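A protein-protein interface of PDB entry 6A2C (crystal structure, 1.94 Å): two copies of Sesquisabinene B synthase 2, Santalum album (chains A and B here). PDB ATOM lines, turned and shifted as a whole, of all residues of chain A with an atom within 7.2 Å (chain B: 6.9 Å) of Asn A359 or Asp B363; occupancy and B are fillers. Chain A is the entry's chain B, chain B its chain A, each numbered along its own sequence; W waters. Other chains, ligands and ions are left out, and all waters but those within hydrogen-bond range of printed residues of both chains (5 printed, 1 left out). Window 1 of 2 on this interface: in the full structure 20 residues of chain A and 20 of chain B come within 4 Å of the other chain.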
ATOM      1  N   TRP A 266      -5.511  20.256  16.807  1.00  0.00           N
ATOM      2  CA  TRP A 266      -6.576  21.194  17.245  1.00  0.00           C
ATOM      3  C   TRP A 266      -5.981  22.215  18.212  1.00  0.00           C
ATOM      4  O   TRP A 266      -6.160  23.450  18.000  1.00  0.00           O
ATOM      5  CB  TRP A 266      -7.760  20.439  17.874  1.00  0.00           C
ATOM      6  CG  TRP A 266      -8.748  21.347  18.541  1.00  0.00           C
ATOM      7  CD1 TRP A 266      -9.650  22.172  17.929  1.00  0.00           C
ATOM      8  CD2 TRP A 266      -8.886  21.584  19.954  1.00  0.00           C
ATOM      9  NE1 TRP A 266     -10.315  22.920  18.854  1.00  0.00           N
ATOM     10  CE2 TRP A 266      -9.902  22.546  20.111  1.00  0.00           C
ATOM     11  CE3 TRP A 266      -8.269  21.062  21.101  1.00  0.00           C
ATOM     12  CZ2 TRP A 266     -10.325  22.982  21.366  1.00  0.00           C
ATOM     13  CZ3 TRP A 266      -8.700  21.486  22.338  1.00  0.00           C
ATOM     14  CH2 TRP A 266      -9.701  22.441  22.471  1.00  0.00           C
ATOM     15  N   GLY A 269      -3.683  24.609  16.733  1.00  0.00           N
ATOM     16  CA  GLY A 269      -4.542  25.464  15.885  1.00  0.00           C
ATOM     17  C   GLY A 269      -5.271  26.535  16.672  1.00  0.00           C
ATOM     18  O   GLY A 269      -5.551  27.621  16.109  1.00  0.00           O
ATOM     19  N   LEU A 311     -10.265  23.383  27.826  1.00  0.00           N
ATOM     20  CA  LEU A 311     -10.760  24.764  27.960  1.00  0.00           C
ATOM     21  C   LEU A 311     -11.054  25.082  29.433  1.00  0.00           C
ATOM     22  O   LEU A 311     -10.955  26.251  29.800  1.00  0.00           O
ATOM     23  CB  LEU A 311     -11.996  24.950  27.074  1.00  0.00           C
ATOM     24  CG  LEU A 311     -11.675  24.951  25.579  1.00  0.00           C
ATOM     25  CD1 LEU A 311     -12.937  25.019  24.728  1.00  0.00           C
ATOM     26  CD2 LEU A 311     -10.742  26.089  25.253  1.00  0.00           C
ATOM     27  N   TRP A 338     -24.142  34.703  24.591  1.00  0.00           N
ATOM     28  CA  TRP A 338     -23.663  33.972  23.377  1.00  0.00           C
ATOM     29  C   TRP A 338     -23.607  34.941  22.193  1.00  0.00           C
ATOM     30  O   TRP A 338     -24.150  34.633  21.109  1.00  0.00           O
ATOM     31  CB  TRP A 338     -24.536  32.759  23.063  1.00  0.00           C
ATOM     32  CG  TRP A 338     -23.779  31.589  22.518  1.00  0.00           C
ATOM     33  CD1 TRP A 338     -23.946  30.991  21.304  1.00  0.00           C
ATOM     34  CD2 TRP A 338     -22.720  30.877  23.176  1.00  0.00           C
ATOM     35  NE1 TRP A 338     -23.084  29.935  21.176  1.00  0.00           N
ATOM     36  CE2 TRP A 338     -22.318  29.844  22.309  1.00  0.00           C
ATOM     37  CE3 TRP A 338     -22.093  30.994  24.420  1.00  0.00           C
ATOM     38  CZ2 TRP A 338     -21.312  28.940  22.648  1.00  0.00           C
ATOM     39  CZ3 TRP A 338     -21.106  30.098  24.757  1.00  0.00           C
ATOM     40  CH2 TRP A 338     -20.716  29.085  23.880  1.00  0.00           C
ATOM     41  N   ILE A 340     -20.616  37.450  20.416  1.00  0.00           N
ATOM     42  CA  ILE A 340     -19.153  37.725  20.427  1.00  0.00           C
ATOM     43  C   ILE A 340     -18.899  39.098  19.805  1.00  0.00           C
ATOM     44  O   ILE A 340     -17.738  39.426  19.566  1.00  0.00           O
ATOM     45  CB  ILE A 340     -18.378  36.600  19.736  1.00  0.00           C
ATOM     46  CG1 ILE A 340     -18.810  36.381  18.284  1.00  0.00           C
ATOM     47  CG2 ILE A 340     -18.484  35.328  20.554  1.00  0.00           C
ATOM     48  CD1 ILE A 340     -17.754  35.695  17.436  1.00  0.00           C
ATOM     49  N   PRO A 353      -8.934  32.373  24.484  1.00  0.00           N
ATOM     50  CA  PRO A 353      -9.704  31.406  25.261  1.00  0.00           C
ATOM     51  C   PRO A 353     -11.212  31.585  25.014  1.00  0.00           C
ATOM     52  O   PRO A 353     -11.912  30.610  24.897  1.00  0.00           O
ATOM     53  CB  PRO A 353      -9.303  31.713  26.718  1.00  0.00           C
ATOM     54  CG  PRO A 353      -7.915  32.292  26.587  1.00  0.00           C
ATOM     55  CD  PRO A 353      -7.961  33.113  25.310  1.00  0.00           C
ATOM     56  N   LEU A 354     -11.689  32.817  24.995  1.00  0.00           N
ATOM     57  CA  LEU A 354     -13.145  33.080  24.893  1.00  0.00           C
ATOM     58  C   LEU A 354     -13.658  32.521  23.558  1.00  0.00           C
ATOM     59  O   LEU A 354     -14.676  31.841  23.541  1.00  0.00           O
ATOM     60  CB  LEU A 354     -13.407  34.579  24.972  1.00  0.00           C
ATOM     61  CG  LEU A 354     -14.831  34.978  24.592  1.00  0.00           C
ATOM     62  CD1 LEU A 354     -15.787  34.498  25.657  1.00  0.00           C
ATOM     63  CD2 LEU A 354     -14.949  36.468  24.378  1.00  0.00           C
ATOM     64  N   LEU A 355     -12.983  32.843  22.465  1.00  0.00           N
ATOM     65  CA  LEU A 355     -13.511  32.515  21.117  1.00  0.00           C
ATOM     66  C   LEU A 355     -13.305  31.030  20.888  1.00  0.00           C
ATOM     67  O   LEU A 355     -14.169  30.422  20.255  1.00  0.00           O
ATOM     68  CB  LEU A 355     -12.846  33.381  20.045  1.00  0.00           C
ATOM     69  CG  LEU A 355     -13.219  34.856  20.082  1.00  0.00           C
ATOM     70  CD1 LEU A 355     -12.434  35.626  19.032  1.00  0.00           C
ATOM     71  CD2 LEU A 355     -14.706  35.055  19.882  1.00  0.00           C
ATOM     72  N   THR A 356     -12.301  30.423  21.519  1.00  0.00           N
ATOM     73  CA  THR A 356     -12.115  28.960  21.422  1.00  0.00           C
ATOM     74  C   THR A 356     -13.238  28.233  22.179  1.00  0.00           C
ATOM     75  O   THR A 356     -13.742  27.206  21.672  1.00  0.00           O
ATOM     76  CB  THR A 356     -10.698  28.538  21.809  1.00  0.00           C
ATOM     77  OG1 THR A 356      -9.745  29.108  20.908  1.00  0.00           O
ATOM     78  CG2 THR A 356     -10.562  27.044  21.771  1.00  0.00           C
ATOM     79  N   MET A 357     -13.601  28.706  23.361  1.00  0.00           N
ATOM     80  CA  MET A 357     -14.753  28.176  24.124  1.00  0.00           C
ATOM     81  C   MET A 357     -16.049  28.257  23.277  1.00  0.00           C
ATOM     82  O   MET A 357     -16.836  27.314  23.275  1.00  0.00           O
ATOM     83  CB  MET A 357     -14.926  28.998  25.400  1.00  0.00           C
ATOM     84  CG  MET A 357     -16.161  28.631  26.213  1.00  0.00           C
ATOM     85  SD  MET A 357     -16.702  30.032  27.229  1.00  0.00           S
ATOM     86  CE  MET A 357     -17.455  31.059  25.967  1.00  0.00           C
ATOM     87  N   PHE A 358     -16.289  29.399  22.688  1.00  0.00           N
ATOM     88  CA  PHE A 358     -17.465  29.687  21.822  1.00  0.00           C
ATOM     89  C   PHE A 358     -17.484  28.718  20.639  1.00  0.00           C
ATOM     90  O   PHE A 358     -18.498  28.022  20.432  1.00  0.00           O
ATOM     91  CB  PHE A 358     -17.392  31.140  21.396  1.00  0.00           C
ATOM     92  CG  PHE A 358     -18.545  31.613  20.557  1.00  0.00           C
ATOM     93  CD1 PHE A 358     -19.776  31.883  21.130  1.00  0.00           C
ATOM     94  CD2 PHE A 358     -18.376  31.847  19.200  1.00  0.00           C
ATOM     95  CE1 PHE A 358     -20.836  32.320  20.354  1.00  0.00           C
ATOM     96  CE2 PHE A 358     -19.438  32.293  18.430  1.00  0.00           C
ATOM     97  CZ  PHE A 358     -20.653  32.565  19.019  1.00  0.00           C
ATOM     98  N   ASN A 359     -16.357  28.638  19.920  1.00  0.00           N
ATOM     99  CA  ASN A 359     -16.253  27.856  18.673  1.00  0.00           C
ATOM    100  C   ASN A 359     -16.348  26.364  18.988  1.00  0.00           C
ATOM    101  O   ASN A 359     -17.135  25.637  18.297  1.00  0.00           O
ATOM    102  CB  ASN A 359     -14.991  28.211  17.900  1.00  0.00           C
ATOM    103  CG  ASN A 359     -15.010  29.585  17.280  1.00  0.00           C
ATOM    104  OD1 ASN A 359     -16.037  30.263  17.203  1.00  0.00           O
ATOM    105  ND2 ASN A 359     -13.860  29.990  16.782  1.00  0.00           N
ATOM    106  N   THR A 360     -15.712  25.916  20.068  1.00  0.00           N
ATOM    107  CA  THR A 360     -15.764  24.499  20.483  1.00  0.00           C
ATOM    108  C   THR A 360     -17.168  24.129  20.976  1.00  0.00           C
ATOM    109  O   THR A 360     -17.650  23.025  20.625  1.00  0.00           O
ATOM    110  CB  THR A 360     -14.702  24.200  21.547  1.00  0.00           C
ATOM    111  OG1 THR A 360     -13.462  24.430  20.888  1.00  0.00           O
ATOM    112  CG2 THR A 360     -14.808  22.789  22.069  1.00  0.00           C
ATOM    113  N   SER A 361     -17.811  25.001  21.729  1.00  0.00           N
ATOM    114  CA  SER A 361     -19.162  24.737  22.280  1.00  0.00           C
ATOM    115  C   SER A 361     -20.157  24.634  21.122  1.00  0.00           C
ATOM    116  O   SER A 361     -21.021  23.744  21.147  1.00  0.00           O
ATOM    117  CB  SER A 361     -19.574  25.799  23.241  1.00  0.00           C
ATOM    118  OG  SER A 361     -18.760  25.780  24.414  1.00  0.00           O
ATOM    119  N   ASN A 362     -20.008  25.516  20.132  1.00  0.00           N
ATOM    120  CA  ASN A 362     -20.791  25.481  18.875  1.00  0.00           C
ATOM    121  C   ASN A 362     -20.527  24.172  18.161  1.00  0.00           C
ATOM    122  O   ASN A 362     -21.498  23.568  17.719  1.00  0.00           O
ATOM    123  CB  ASN A 362     -20.502  26.696  18.010  1.00  0.00           C
ATOM    124  CG  ASN A 362     -21.051  27.958  18.632  1.00  0.00           C
ATOM    125  OD1 ASN A 362     -22.022  27.905  19.375  1.00  0.00           O
ATOM    126  ND2 ASN A 362     -20.495  29.097  18.273  1.00  0.00           N
ATOM    127  N   ASP A 363     -19.268  23.730  18.057  1.00  0.00           N
ATOM    128  CA  ASP A 363     -18.944  22.459  17.368  1.00  0.00           C
ATOM    129  C   ASP A 363     -19.575  21.266  18.106  1.00  0.00           C
ATOM    130  O   ASP A 363     -20.099  20.347  17.436  1.00  0.00           O
ATOM    131  CB  ASP A 363     -17.444  22.203  17.265  1.00  0.00           C
ATOM    132  CG  ASP A 363     -16.656  23.071  16.301  1.00  0.00           C
ATOM    133  OD1 ASP A 363     -17.237  23.583  15.296  1.00  0.00           O
ATOM    134  OD2 ASP A 363     -15.433  23.187  16.544  1.00  0.00           O
ATOM    135  N   ILE A 364     -19.516  21.232  19.432  1.00  0.00           N
ATOM    136  CA  ILE A 364     -20.033  20.050  20.178  1.00  0.00           C
ATOM    137  C   ILE A 364     -21.574  20.028  20.090  1.00  0.00           C
ATOM    138  O   ILE A 364     -22.128  18.969  19.811  1.00  0.00           O
ATOM    139  CB  ILE A 364     -19.518  20.054  21.623  1.00  0.00           C
ATOM    140  CG1 ILE A 364     -18.004  19.854  21.676  1.00  0.00           C
ATOM    141  CG2 ILE A 364     -20.275  19.002  22.432  1.00  0.00           C
ATOM    142  CD1 ILE A 364     -17.380  20.212  23.014  1.00  0.00           C
ATOM    143  N   GLY A 365     -22.219  21.167  20.286  1.00  0.00           N
ATOM    144  CA  GLY A 365     -23.660  21.345  20.036  1.00  0.00           C
ATOM    145  C   GLY A 365     -24.046  20.847  18.658  1.00  0.00           C
ATOM    146  O   GLY A 365     -25.049  20.117  18.508  1.00  0.00           O
ATOM    147  N   TRP B 266     -13.288  16.573   7.709  1.00  0.00           N
ATOM    148  CA  TRP B 266     -14.098  17.733   8.149  1.00  0.00           C
ATOM    149  C   TRP B 266     -15.512  17.613   7.535  1.00  0.00           C
ATOM    150  O   TRP B 266     -16.498  17.762   8.277  1.00  0.00           O
ATOM    151  CB  TRP B 266     -13.399  19.045   7.777  1.00  0.00           C
ATOM    152  CG  TRP B 266     -14.295  20.238   7.832  1.00  0.00           C
ATOM    153  CD1 TRP B 266     -14.689  20.907   8.952  1.00  0.00           C
ATOM    154  CD2 TRP B 266     -14.990  20.840   6.729  1.00  0.00           C
ATOM    155  NE1 TRP B 266     -15.537  21.920   8.622  1.00  0.00           N
ATOM    156  CE2 TRP B 266     -15.739  21.905   7.263  1.00  0.00           C
ATOM    157  CE3 TRP B 266     -14.999  20.627   5.347  1.00  0.00           C
ATOM    158  CZ2 TRP B 266     -16.482  22.765   6.458  1.00  0.00           C
ATOM    159  CZ3 TRP B 266     -15.732  21.478   4.549  1.00  0.00           C
ATOM    160  CH2 TRP B 266     -16.467  22.529   5.100  1.00  0.00           C
ATOM    161  N   MET B 304      -8.888  26.380   3.841  1.00  0.00           N
ATOM    162  CA  MET B 304      -9.980  27.279   4.281  1.00  0.00           C
ATOM    163  C   MET B 304     -10.786  27.727   3.054  1.00  0.00           C
ATOM    164  O   MET B 304     -12.021  27.784   3.143  1.00  0.00           O
ATOM    165  CB  MET B 304      -9.427  28.445   5.085  1.00  0.00           C
ATOM    166  CG  MET B 304      -9.070  28.004   6.517  1.00  0.00           C
ATOM    167  SD  MET B 304      -8.447  29.302   7.560  1.00  0.00           S
ATOM    168  CE  MET B 304      -6.726  29.363   7.062  1.00  0.00           C
ATOM    169  N   LYS B 307     -13.078  24.964   2.057  1.00  0.00           N
ATOM    170  CA  LYS B 307     -14.233  24.867   2.980  1.00  0.00           C
ATOM    171  C   LYS B 307     -15.289  25.907   2.583  1.00  0.00           C
ATOM    172  O   LYS B 307     -16.473  25.557   2.504  1.00  0.00           O
ATOM    173  CB  LYS B 307     -13.820  25.095   4.425  1.00  0.00           C
ATOM    174  CG  LYS B 307     -13.019  23.969   5.063  1.00  0.00           C
ATOM    175  CD  LYS B 307     -12.674  24.272   6.478  1.00  0.00           C
ATOM    176  CE  LYS B 307     -12.058  23.098   7.199  1.00  0.00           C
ATOM    177  NZ  LYS B 307     -11.823  23.490   8.590  1.00  0.00           N
ATOM    178  N   THR B 356     -23.135  25.110   9.887  1.00  0.00           N
ATOM    179  CA  THR B 356     -21.776  24.844   9.376  1.00  0.00           C
ATOM    180  C   THR B 356     -21.182  26.136   8.800  1.00  0.00           C
ATOM    181  O   THR B 356     -19.992  26.443   9.099  1.00  0.00           O
ATOM    182  CB  THR B 356     -21.743  23.651   8.427  1.00  0.00           C
ATOM    183  OG1 THR B 356     -22.265  22.536   9.161  1.00  0.00           O
ATOM    184  CG2 THR B 356     -20.333  23.410   7.925  1.00  0.00           C
ATOM    185  N   MET B 357     -21.949  26.901   8.029  1.00  0.00           N
ATOM    186  CA  MET B 357     -21.492  28.241   7.553  1.00  0.00           C
ATOM    187  C   MET B 357     -21.019  29.069   8.750  1.00  0.00           C
ATOM    188  O   MET B 357     -19.938  29.660   8.680  1.00  0.00           O
ATOM    189  CB  MET B 357     -22.598  28.981   6.793  1.00  0.00           C
ATOM    190  CG  MET B 357     -22.293  30.469   6.471  1.00  0.00           C
ATOM    191  SD  MET B 357     -23.836  31.349   6.227  1.00  0.00           S
ATOM    192  CE  MET B 357     -24.342  31.465   7.946  1.00  0.00           C
ATOM    193  N   PHE B 358     -21.842  29.157   9.783  1.00  0.00           N
ATOM    194  CA  PHE B 358     -21.586  29.948  11.016  1.00  0.00           C
ATOM    195  C   PHE B 358     -20.298  29.440  11.688  1.00  0.00           C
ATOM    196  O   PHE B 358     -19.397  30.236  11.908  1.00  0.00           O
ATOM    197  CB  PHE B 358     -22.819  29.852  11.932  1.00  0.00           C
ATOM    198  CG  PHE B 358     -22.744  30.638  13.204  1.00  0.00           C
ATOM    199  CD1 PHE B 358     -22.900  32.014  13.185  1.00  0.00           C
ATOM    200  CD2 PHE B 358     -22.511  30.008  14.417  1.00  0.00           C
ATOM    201  CE1 PHE B 358     -22.813  32.750  14.356  1.00  0.00           C
ATOM    202  CE2 PHE B 358     -22.470  30.744  15.595  1.00  0.00           C
ATOM    203  CZ  PHE B 358     -22.650  32.105  15.557  1.00  0.00           C
ATOM    204  N   ASN B 359     -20.197  28.141  11.955  1.00  0.00           N
ATOM    205  CA  ASN B 359     -19.056  27.545  12.710  1.00  0.00           C
ATOM    206  C   ASN B 359     -17.764  27.709  11.905  1.00  0.00           C
ATOM    207  O   ASN B 359     -16.743  28.073  12.495  1.00  0.00           O
ATOM    208  CB  ASN B 359     -19.298  26.080  13.101  1.00  0.00           C
ATOM    209  CG  ASN B 359     -20.368  25.921  14.156  1.00  0.00           C
ATOM    210  OD1 ASN B 359     -20.799  26.889  14.761  1.00  0.00           O
ATOM    211  ND2 ASN B 359     -20.841  24.710  14.364  1.00  0.00           N
ATOM    212  N   THR B 360     -17.799  27.466  10.598  1.00  0.00           N
ATOM    213  CA  THR B 360     -16.612  27.562   9.723  1.00  0.00           C
ATOM    214  C   THR B 360     -16.166  29.019   9.595  1.00  0.00           C
ATOM    215  O   THR B 360     -14.906  29.287   9.708  1.00  0.00           O
ATOM    216  CB  THR B 360     -16.881  26.910   8.367  1.00  0.00           C
ATOM    217  OG1 THR B 360     -17.090  25.517   8.579  1.00  0.00           O
ATOM    218  CG2 THR B 360     -15.756  27.132   7.390  1.00  0.00           C
ATOM    219  N   SER B 361     -17.114  29.940   9.425  1.00  0.00           N
ATOM    220  CA  SER B 361     -16.821  31.392   9.370  1.00  0.00           C
ATOM    221  C   SER B 361     -16.141  31.829  10.674  1.00  0.00           C
ATOM    222  O   SER B 361     -15.184  32.560  10.577  1.00  0.00           O
ATOM    223  CB  SER B 361     -18.028  32.222   9.064  1.00  0.00           C
ATOM    224  OG  SER B 361     -18.502  31.822   7.788  1.00  0.00           O
ATOM    225  N   ASN B 362     -16.657  31.409  11.826  1.00  0.00           N
ATOM    226  CA  ASN B 362     -16.024  31.681  13.143  1.00  0.00           C
ATOM    227  C   ASN B 362     -14.632  31.053  13.194  1.00  0.00           C
ATOM    228  O   ASN B 362     -13.737  31.743  13.674  1.00  0.00           O
ATOM    229  CB  ASN B 362     -16.907  31.238  14.293  1.00  0.00           C
ATOM    230  CG  ASN B 362     -18.202  32.006  14.326  1.00  0.00           C
ATOM    231  OD1 ASN B 362     -18.252  33.137  13.864  1.00  0.00           O
ATOM    232  ND2 ASN B 362     -19.224  31.415  14.906  1.00  0.00           N
ATOM    233  N   ASP B 363     -14.453  29.817  12.736  1.00  0.00           N
ATOM    234  CA  ASP B 363     -13.134  29.151  12.705  1.00  0.00           C
ATOM    235  C   ASP B 363     -12.150  29.954  11.837  1.00  0.00           C
ATOM    236  O   ASP B 363     -10.980  30.181  12.277  1.00  0.00           O
ATOM    237  CB  ASP B 363     -13.212  27.735  12.159  1.00  0.00           C
ATOM    238  CG  ASP B 363     -13.794  26.701  13.089  1.00  0.00           C
ATOM    239  OD1 ASP B 363     -13.960  26.998  14.279  1.00  0.00           O
ATOM    240  OD2 ASP B 363     -14.186  25.639  12.566  1.00  0.00           O
ATOM    241  N   ILE B 364     -12.571  30.387  10.652  1.00  0.00           N
ATOM    242  CA  ILE B 364     -11.681  31.115   9.700  1.00  0.00           C
ATOM    243  C   ILE B 364     -11.306  32.466  10.299  1.00  0.00           C
ATOM    244  O   ILE B 364     -10.114  32.803  10.289  1.00  0.00           O
ATOM    245  CB  ILE B 364     -12.291  31.208   8.289  1.00  0.00           C
ATOM    246  CG1 ILE B 364     -12.333  29.827   7.652  1.00  0.00           C
ATOM    247  CG2 ILE B 364     -11.508  32.170   7.434  1.00  0.00           C
ATOM    248  CD1 ILE B 364     -13.158  29.725   6.387  1.00  0.00           C
ATOM    249  N   GLY B 365     -12.273  33.212  10.817  1.00  0.00           N
ATOM    250  CA  GLY B 365     -12.016  34.496  11.474  1.00  0.00           C
ATOM    251  C   GLY B 365     -11.053  34.326  12.644  1.00  0.00           C
ATOM    252  O   GLY B 365     -10.228  35.220  12.874  1.00  0.00           O
ATOM    253  N   TYR B 366     -11.200  33.243  13.399  1.00  0.00           N
ATOM    254  CA  TYR B 366     -10.361  32.954  14.588  1.00  0.00           C
ATOM    255  C   TYR B 366      -8.930  32.632  14.129  1.00  0.00           C
ATOM    256  O   TYR B 366      -7.966  33.045  14.808  1.00  0.00           O
ATOM    257  CB  TYR B 366     -10.959  31.842  15.444  1.00  0.00           C
ATOM    258  CG  TYR B 366     -10.104  31.542  16.646  1.00  0.00           C
ATOM    259  CD1 TYR B 366      -9.010  30.708  16.552  1.00  0.00           C
ATOM    260  CD2 TYR B 366     -10.332  32.193  17.842  1.00  0.00           C
ATOM    261  CE1 TYR B 366      -8.202  30.457  17.652  1.00  0.00           C
ATOM    262  CE2 TYR B 366      -9.556  31.935  18.960  1.00  0.00           C
ATOM    263  CZ  TYR B 366      -8.459  31.100  18.848  1.00  0.00           C
ATOM    264  OH  TYR B 366      -7.663  30.869  19.924  1.00  0.00           O
ATOM    265  N   TRP B 367      -8.766  31.905  13.034  1.00  0.00           N
ATOM    266  CA  TRP B 367      -7.421  31.625  12.475  1.00  0.00           C
ATOM    267  C   TRP B 367      -6.689  32.954  12.220  1.00  0.00           C
ATOM    268  O   TRP B 367      -5.485  33.054  12.573  1.00  0.00           O
ATOM    269  CB  TRP B 367      -7.520  30.783  11.218  1.00  0.00           C
ATOM    270  CG  TRP B 367      -6.211  30.316  10.664  1.00  0.00           C
ATOM    271  CD1 TRP B 367      -5.668  29.079  10.797  1.00  0.00           C
ATOM    272  CD2 TRP B 367      -5.314  31.056   9.815  1.00  0.00           C
ATOM    273  NE1 TRP B 367      -4.517  28.981  10.067  1.00  0.00           N
ATOM    274  CE2 TRP B 367      -4.269  30.184   9.459  1.00  0.00           C
ATOM    275  CE3 TRP B 367      -5.336  32.336   9.268  1.00  0.00           C
ATOM    276  CZ2 TRP B 367      -3.221  30.573   8.624  1.00  0.00           C
ATOM    277  CZ3 TRP B 367      -4.307  32.722   8.437  1.00  0.00           C
ATOM    278  CH2 TRP B 367      -3.274  31.843   8.106  1.00  0.00           C
ATOM    279  N   ALA B 368      -7.358  33.945  11.631  1.00  0.00           N
ATOM    280  CA  ALA B 368      -6.753  35.267  11.380  1.00  0.00           C
ATOM    281  C   ALA B 368      -6.341  35.914  12.712  1.00  0.00           C
ATOM    282  O   ALA B 368      -5.279  36.575  12.753  1.00  0.00           O
ATOM    283  CB  ALA B 368      -7.687  36.151  10.605  1.00  0.00           C
ATOM    284  N   ILE B 377     -13.619  37.524  12.177  1.00  0.00           N
ATOM    285  CA  ILE B 377     -15.034  37.044  12.245  1.00  0.00           C
ATOM    286  C   ILE B 377     -15.975  38.102  11.690  1.00  0.00           C
ATOM    287  O   ILE B 377     -16.889  37.784  10.929  1.00  0.00           O
ATOM    288  CB  ILE B 377     -15.403  36.574  13.662  1.00  0.00           C
ATOM    289  CG1 ILE B 377     -14.543  35.365  14.017  1.00  0.00           C
ATOM    290  CG2 ILE B 377     -16.902  36.292  13.765  1.00  0.00           C
ATOM    291  CD1 ILE B 377     -14.807  34.779  15.374  1.00  0.00           C
ATOM    292  N   THR B 380     -15.696  37.687   7.772  1.00  0.00           N
ATOM    293  CA  THR B 380     -16.326  36.473   7.204  1.00  0.00           C
ATOM    294  C   THR B 380     -17.836  36.602   7.395  1.00  0.00           C
ATOM    295  O   THR B 380     -18.556  36.291   6.454  1.00  0.00           O
ATOM    296  CB  THR B 380     -15.708  35.188   7.767  1.00  0.00           C
ATOM    297  OG1 THR B 380     -15.968  35.135   9.168  1.00  0.00           O
ATOM    298  CG2 THR B 380     -14.213  35.113   7.536  1.00  0.00           C
HETATM  299  O   HOH W   1     -13.723  25.345  16.255  1.00  0.00           O
HETATM  300  O   HOH W   2     -19.066  22.061  13.662  1.00  0.00           O
HETATM  301  O   HOH W   3     -16.275  24.114  13.043  1.00  0.00           O
HETATM  302  O   HOH W   4     -18.692  28.774  16.095  1.00  0.00           O
HETATM  303  O   HOH W   5     -11.661  27.937  15.743  1.00  0.00           O
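The side-chain hydroxyl (OG1) of Thr A356 is in hydrogen-bond range of the side-chain hydroxyl (OH) of Tyr B366 (2.9 Å).
O of Ile B377 sits at hydrogen-bond distance from OG1 of Thr B380 (3.3 Å). The backbone carbonyl oxygen of Thr A356 lies within hydrogen-bond range of the side-chain hydroxyl of Thr A360 (2.9 Å). OD1 of Asn A362 lies within hydrogen-bond range of NE1 of Trp A338 (2.9 Å). ND2 of Asn B362 lies close to O of Phe B358. The backbone carbonyl oxygen (O) of Phe A358 lies close to the side-chain amide nitrogen (ND2) of Asn A362, 3.1 Å away.
Among the printed residues, merely in contact across the chains: Asn A359 with Asn B362 (3.2 Å), Asn A362 with Asn B359 (3.3 Å), Leu A355 with Tyr B366 (3.5 Å), Phe A358 with Asn B362 (3.6 Å), Asn A359 with Tyr B366 (3.7 Å), Ile A340 with Ile B377 (3.7 Å), Asn A362 with Phe B358 (3.7 Å), Asp A363 with Asn B359 (3.9 Å) and Asn A359 with Asp B363 (3.9 Å).
Asn A359 touches just these residues of chain B: Asn B362 (3.2 Å), Asp B363 (3.9 Å) and Tyr B366 (3.7 Å). Printed residues of chain A within 4 Å of Asp B363: Asn A359 (3.9 Å). Printed residues of chain A within 4 Å of Asn B359: Asn A362 (3.3 Å) and Asp A363 (3.9 Å). Printed residues of chain A within 4 Å of Ile B377: Ile A340. Of the printed residues of chain B, Asp A363 touches Asn B359 (3.9 Å). Of the printed residues of chain B, Ile A340 touches Ile B377. Ile A364 touches none of the printed residues of chain B. Met A357 touches none of the printed residues of chain B.
Of the 18 printed residues of chain A, 7 touch a printed residue of chain B. Hydrophobic or aromatic side chains of chain A that line the printed part of chain B: Ile A340, Leu A355 and Phe A358. Of the 18 printed residues of chain B, 6 touch a printed residue of chain A. Hydrophobic or aromatic side chains of chain B that line the printed part of chain A: Phe B358, Tyr B366 and Ile B377. Among the printed residues, no Asp or Glu carboxylate lies within 4 Å of a Lys or Arg side-chain nitrogen of the other chain.
Phe A358 touches Asn B362, and with the chains exchanged Asn A362 touches Phe B358. Asn A359 touches Asn B362, and with the chains exchanged Asn A362 touches Asn B359. Asn A359 touches Asp B363, and with the chains exchanged Asp A363 touches Asn B359. 11 positions are printed for both chains. Of the 10 pairs that touch across the chains among the printed residues, 6 have their exchanged pair printed and touching as well.
Water W3 lies within hydrogen-bond range of the side-chain carboxylate (OD1) of Asp A363 (2.5 Å) and the side-chain carboxylate (OD2) of Asp B363 (2.6 Å). Water W1 bridges OD1 of Asp B363 (2.6 Å) and OD2 of Asp A363 (2.8 Å). Water W4 lies within hydrogen-bond range of ND2 of Asn A362 (2.8 Å), ND2 of Asn B362 (2.9 Å), OD1 of Asn B359 (3.1 Å) and OD1 of Asn A359 (3.2 Å). Water W5 lies within hydrogen-bond range of OD1 of Asp B363 (2.9 Å) and ND2 of Asn A359 (3.2 Å). Water W2 bridges OD1 of Asp A363 (2.9 Å) and ND2 of Asn B359 (3.3 Å).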
